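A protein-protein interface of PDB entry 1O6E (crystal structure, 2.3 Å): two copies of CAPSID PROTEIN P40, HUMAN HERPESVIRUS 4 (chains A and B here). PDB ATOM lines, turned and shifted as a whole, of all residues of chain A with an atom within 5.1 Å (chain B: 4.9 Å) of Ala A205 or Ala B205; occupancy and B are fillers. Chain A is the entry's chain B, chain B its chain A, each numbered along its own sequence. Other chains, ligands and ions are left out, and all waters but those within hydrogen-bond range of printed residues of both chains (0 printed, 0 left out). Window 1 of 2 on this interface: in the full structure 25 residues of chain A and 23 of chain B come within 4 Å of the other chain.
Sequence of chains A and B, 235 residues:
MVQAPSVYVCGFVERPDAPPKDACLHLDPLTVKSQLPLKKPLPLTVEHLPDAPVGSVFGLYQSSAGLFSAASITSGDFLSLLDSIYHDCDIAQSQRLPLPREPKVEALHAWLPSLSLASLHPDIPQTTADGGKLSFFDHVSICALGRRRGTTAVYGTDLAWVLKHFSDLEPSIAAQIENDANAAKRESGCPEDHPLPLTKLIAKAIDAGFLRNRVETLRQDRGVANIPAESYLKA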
ATOM      1  N   LEU A 201     -16.885   4.076 -35.259  1.00  0.00           N
ATOM      2  CA  LEU A 201     -16.911   2.775 -34.585  1.00  0.00           C
ATOM      3  C   LEU A 201     -16.633   2.921 -33.094  1.00  0.00           C
ATOM      4  O   LEU A 201     -17.216   2.217 -32.278  1.00  0.00           O
ATOM      5  CB  LEU A 201     -15.874   1.814 -35.207  1.00  0.00           C
ATOM      6  CG  LEU A 201     -15.970   1.417 -36.689  1.00  0.00           C
ATOM      7  CD1 LEU A 201     -14.807   0.495 -37.008  1.00  0.00           C
ATOM      8  CD2 LEU A 201     -17.303   0.728 -37.005  1.00  0.00           C
ATOM      9  N   ILE A 202     -15.735   3.830 -32.741  1.00  0.00           N
ATOM     10  CA  ILE A 202     -15.407   4.058 -31.344  1.00  0.00           C
ATOM     11  C   ILE A 202     -16.648   4.649 -30.658  1.00  0.00           C
ATOM     12  O   ILE A 202     -17.014   4.241 -29.556  1.00  0.00           O
ATOM     13  CB  ILE A 202     -14.175   5.012 -31.211  1.00  0.00           C
ATOM     14  CG1 ILE A 202     -13.360   4.663 -29.963  1.00  0.00           C
ATOM     15  CG2 ILE A 202     -14.615   6.457 -31.167  1.00  0.00           C
ATOM     16  CD1 ILE A 202     -14.160   4.553 -28.698  1.00  0.00           C
ATOM     17  N   ALA A 203     -17.301   5.597 -31.323  1.00  0.00           N
ATOM     18  CA  ALA A 203     -18.506   6.226 -30.794  1.00  0.00           C
ATOM     19  C   ALA A 203     -19.552   5.158 -30.523  1.00  0.00           C
ATOM     20  O   ALA A 203     -20.204   5.161 -29.485  1.00  0.00           O
ATOM     21  CB  ALA A 203     -19.042   7.232 -31.798  1.00  0.00           C
ATOM     22  N   LYS A 204     -19.711   4.249 -31.476  1.00  0.00           N
ATOM     23  CA  LYS A 204     -20.665   3.158 -31.354  1.00  0.00           C
ATOM     24  C   LYS A 204     -20.279   2.250 -30.199  1.00  0.00           C
ATOM     25  O   LYS A 204     -21.139   1.661 -29.564  1.00  0.00           O
ATOM     26  CB  LYS A 204     -20.724   2.373 -32.666  1.00  0.00           C
ATOM     27  CG  LYS A 204     -21.525   3.072 -33.764  1.00  0.00           C
ATOM     28  CD  LYS A 204     -22.995   3.140 -33.384  1.00  0.00           C
ATOM     29  CE  LYS A 204     -23.792   3.987 -34.348  1.00  0.00           C
ATOM     30  NZ  LYS A 204     -25.229   3.962 -33.967  1.00  0.00           N
ATOM     31  N   ALA A 205     -18.981   2.154 -29.928  1.00  0.00           N
ATOM     32  CA  ALA A 205     -18.462   1.333 -28.836  1.00  0.00           C
ATOM     33  C   ALA A 205     -18.696   2.049 -27.513  1.00  0.00           C
ATOM     34  O   ALA A 205     -18.865   1.411 -26.474  1.00  0.00           O
ATOM     35  CB  ALA A 205     -16.959   1.065 -29.031  1.00  0.00           C
ATOM     36  N   ILE A 206     -18.693   3.379 -27.564  1.00  0.00           N
ATOM     37  CA  ILE A 206     -18.922   4.191 -26.373  1.00  0.00           C
ATOM     38  C   ILE A 206     -20.375   4.042 -25.930  1.00  0.00           C
ATOM     39  O   ILE A 206     -20.657   3.913 -24.741  1.00  0.00           O
ATOM     40  CB  ILE A 206     -18.615   5.695 -26.624  1.00  0.00           C
ATOM     41  CG1 ILE A 206     -17.181   5.857 -27.127  1.00  0.00           C
ATOM     42  CG2 ILE A 206     -18.796   6.491 -25.334  1.00  0.00           C
ATOM     43  CD1 ILE A 206     -16.173   5.167 -26.259  1.00  0.00           C
ATOM     44  N   ASP A 207     -21.293   4.053 -26.895  1.00  0.00           N
ATOM     45  CA  ASP A 207     -22.714   3.912 -26.602  1.00  0.00           C
ATOM     46  C   ASP A 207     -22.952   2.588 -25.888  1.00  0.00           C
ATOM     47  O   ASP A 207     -23.833   2.482 -25.020  1.00  0.00           O
ATOM     48  CB  ASP A 207     -23.562   3.951 -27.894  1.00  0.00           C
ATOM     49  CG  ASP A 207     -23.689   5.360 -28.492  1.00  0.00           C
ATOM     50  OD1 ASP A 207     -23.606   6.348 -27.734  1.00  0.00           O
ATOM     51  OD2 ASP A 207     -23.898   5.481 -29.723  1.00  0.00           O
ATOM     52  N   ALA A 208     -22.148   1.590 -26.253  1.00  0.00           N
ATOM     53  CA  ALA A 208     -22.259   0.252 -25.686  1.00  0.00           C
ATOM     54  C   ALA A 208     -21.666   0.148 -24.288  1.00  0.00           C
ATOM     55  O   ALA A 208     -21.562  -0.945 -23.733  1.00  0.00           O
ATOM     56  CB  ALA A 208     -21.600  -0.757 -26.613  1.00  0.00           C
ATOM     57  N   GLY A 209     -21.270   1.285 -23.730  1.00  0.00           N
ATOM     58  CA  GLY A 209     -20.718   1.299 -22.393  1.00  0.00           C
ATOM     59  C   GLY A 209     -21.814   1.641 -21.395  1.00  0.00           C
ATOM     60  O   GLY A 209     -21.676   1.379 -20.196  1.00  0.00           O
ATOM     61  N   LEU B 201      -7.680   1.962 -28.725  1.00  0.00           N
ATOM     62  CA  LEU B 201      -8.705   2.718 -27.996  1.00  0.00           C
ATOM     63  C   LEU B 201     -10.070   2.062 -28.119  1.00  0.00           C
ATOM     64  O   LEU B 201     -10.854   2.078 -27.170  1.00  0.00           O
ATOM     65  CB  LEU B 201      -8.833   4.138 -28.538  1.00  0.00           C
ATOM     66  CG  LEU B 201      -7.649   5.100 -28.468  1.00  0.00           C
ATOM     67  CD1 LEU B 201      -8.040   6.411 -29.134  1.00  0.00           C
ATOM     68  CD2 LEU B 201      -7.256   5.333 -27.028  1.00  0.00           C
ATOM     69  N   ILE B 202     -10.364   1.528 -29.305  1.00  0.00           N
ATOM     70  CA  ILE B 202     -11.634   0.842 -29.540  1.00  0.00           C
ATOM     71  C   ILE B 202     -11.670  -0.399 -28.651  1.00  0.00           C
ATOM     72  O   ILE B 202     -12.662  -0.651 -27.968  1.00  0.00           O
ATOM     73  CB  ILE B 202     -11.820   0.398 -31.026  1.00  0.00           C
ATOM     74  CG1 ILE B 202     -12.370   1.547 -31.878  1.00  0.00           C
ATOM     75  CG2 ILE B 202     -12.851  -0.724 -31.104  1.00  0.00           C
ATOM     76  CD1 ILE B 202     -11.586   2.827 -31.819  1.00  0.00           C
ATOM     77  N   ALA B 203     -10.581  -1.164 -28.661  1.00  0.00           N
ATOM     78  CA  ALA B 203     -10.485  -2.368 -27.841  1.00  0.00           C
ATOM     79  C   ALA B 203     -10.732  -2.011 -26.381  1.00  0.00           C
ATOM     80  O   ALA B 203     -11.430  -2.727 -25.667  1.00  0.00           O
ATOM     81  CB  ALA B 203      -9.117  -2.995 -27.991  1.00  0.00           C
ATOM     82  N   LYS B 204     -10.146  -0.905 -25.938  1.00  0.00           N
ATOM     83  CA  LYS B 204     -10.320  -0.443 -24.567  1.00  0.00           C
ATOM     84  C   LYS B 204     -11.780  -0.101 -24.322  1.00  0.00           C
ATOM     85  O   LYS B 204     -12.287  -0.289 -23.221  1.00  0.00           O
ATOM     86  CB  LYS B 204      -9.458   0.798 -24.291  1.00  0.00           C
ATOM     87  CG  LYS B 204      -7.963   0.526 -24.110  1.00  0.00           C
ATOM     88  CD  LYS B 204      -7.707  -0.365 -22.900  1.00  0.00           C
ATOM     89  CE  LYS B 204      -6.223  -0.624 -22.666  1.00  0.00           C
ATOM     90  NZ  LYS B 204      -6.035  -1.341 -21.375  1.00  0.00           N
ATOM     91  N   ALA B 205     -12.446   0.415 -25.354  1.00  0.00           N
ATOM     92  CA  ALA B 205     -13.857   0.786 -25.274  1.00  0.00           C
ATOM     93  C   ALA B 205     -14.740  -0.467 -25.295  1.00  0.00           C
ATOM     94  O   ALA B 205     -15.841  -0.475 -24.733  1.00  0.00           O
ATOM     95  CB  ALA B 205     -14.209   1.697 -26.420  1.00  0.00           C
ATOM     96  N   ILE B 206     -14.243  -1.517 -25.951  1.00  0.00           N
ATOM     97  CA  ILE B 206     -14.924  -2.812 -26.044  1.00  0.00           C
ATOM     98  C   ILE B 206     -14.973  -3.420 -24.640  1.00  0.00           C
ATOM     99  O   ILE B 206     -16.012  -3.916 -24.207  1.00  0.00           O
ATOM    100  CB  ILE B 206     -14.131  -3.829 -26.942  1.00  0.00           C
ATOM    101  CG1 ILE B 206     -13.866  -3.254 -28.334  1.00  0.00           C
ATOM    102  CG2 ILE B 206     -14.892  -5.148 -27.044  1.00  0.00           C
ATOM    103  CD1 ILE B 206     -15.058  -3.194 -29.211  1.00  0.00           C
ATOM    104  N   ASP B 207     -13.824  -3.395 -23.960  1.00  0.00           N
ATOM    105  CA  ASP B 207     -13.675  -3.928 -22.602  1.00  0.00           C
ATOM    106  C   ASP B 207     -14.696  -3.293 -21.657  1.00  0.00           C
ATOM    107  O   ASP B 207     -15.244  -3.963 -20.769  1.00  0.00           O
ATOM    108  CB  ASP B 207     -12.260  -3.648 -22.065  1.00  0.00           C
ATOM    109  CG  ASP B 207     -11.172  -4.355 -22.863  1.00  0.00           C
ATOM    110  OD1 ASP B 207     -11.509  -4.965 -23.896  1.00  0.00           O
ATOM    111  OD2 ASP B 207      -9.984  -4.297 -22.463  1.00  0.00           O
ATOM    112  N   ALA B 208     -14.931  -1.992 -21.855  1.00  0.00           N
ATOM    113  CA  ALA B 208     -15.870  -1.220 -21.047  1.00  0.00           C
ATOM    114  C   ALA B 208     -17.287  -1.721 -21.280  1.00  0.00           C
ATOM    115  O   ALA B 208     -18.165  -1.519 -20.448  1.00  0.00           O
ATOM    116  CB  ALA B 208     -15.764   0.268 -21.392  1.00  0.00           C
ATOM    117  N   GLY B 209     -17.490  -2.369 -22.423  1.00  0.00           N
ATOM    118  CA  GLY B 209     -18.788  -2.917 -22.767  1.00  0.00           C
ATOM    119  C   GLY B 209     -19.081  -4.142 -21.924  1.00  0.00           C
ATOM    120  O   GLY B 209     -20.207  -4.626 -21.886  1.00  0.00           O
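Ile B202 touches its own counterpart, Ile A202. Ala B205 touches its own counterpart, Ala A205. Ile A206 touches Ala B205, but with the chains exchanged Ala A205 does not touch Ile B206 (4.7 Å). Ala A208 touches Gly B209, but with the chains exchanged Gly A209 does not touch Ala B208 (4.3 Å). Of the 5 pairs that touch across the chains among the printed residues, 2 have their exchanged pair printed and touching as well.
Ile A202 touches Ile B202 (CG1 to CD1, 3.2 Å). CB of Ala B205 touches CD1 of Ile A202, 3.7 Å away. CB of Ala A205 touches CB of Ala B205 (3.8 Å). CB of Ala B205 touches CD1 of Ile A206, at 3.99 Å. O of Ala A208 touches CA of Gly B209 (3.5 Å).
Printed residues of chain A that touch a printed residue of chain B: Ile A202, Ala A205, Ile A206 and Ala A208. Hydrophobic or aromatic side chains of chain A within 4 Å of the printed part of chain B: Ile A202, Ala A205 and Ile A206. Of the 9 printed residues of chain B, 3 touch a printed residue of chain A. Hydrophobic or aromatic side chains of chain B that line the printed part of chain A: Ile B202 and Ala B205. Among the printed residues, 5 pairs touch across the chains. Among the printed residues, no Asp or Glu carboxylate lies within 4 Å of a Lys or Arg side-chain nitrogen of the other chain.
Ala A205 touches just one residue of chain B: Ala B205. Of the printed residues of chain A, Ala B205 touches Ile A202 (3.7 Å), Ala A205 (3.8 Å) and Ile A206 (3.99 Å). Of the printed residues of chain B, Ile A206 touches Ala B205. Printed residues of chain A within 4 Å of Gly B209: Ala A208 (3.5 Å). Printed residues of chain A within 4 Å of Ile B202: Ile A202 (3.2 Å). Ala A203 touches none of the printed residues of chain B. Leu A201 touches none of the printed residues of chain B. The nearest printed residue of chain A that does not touch Ala B205 is Gly A209 (5.7 Å).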
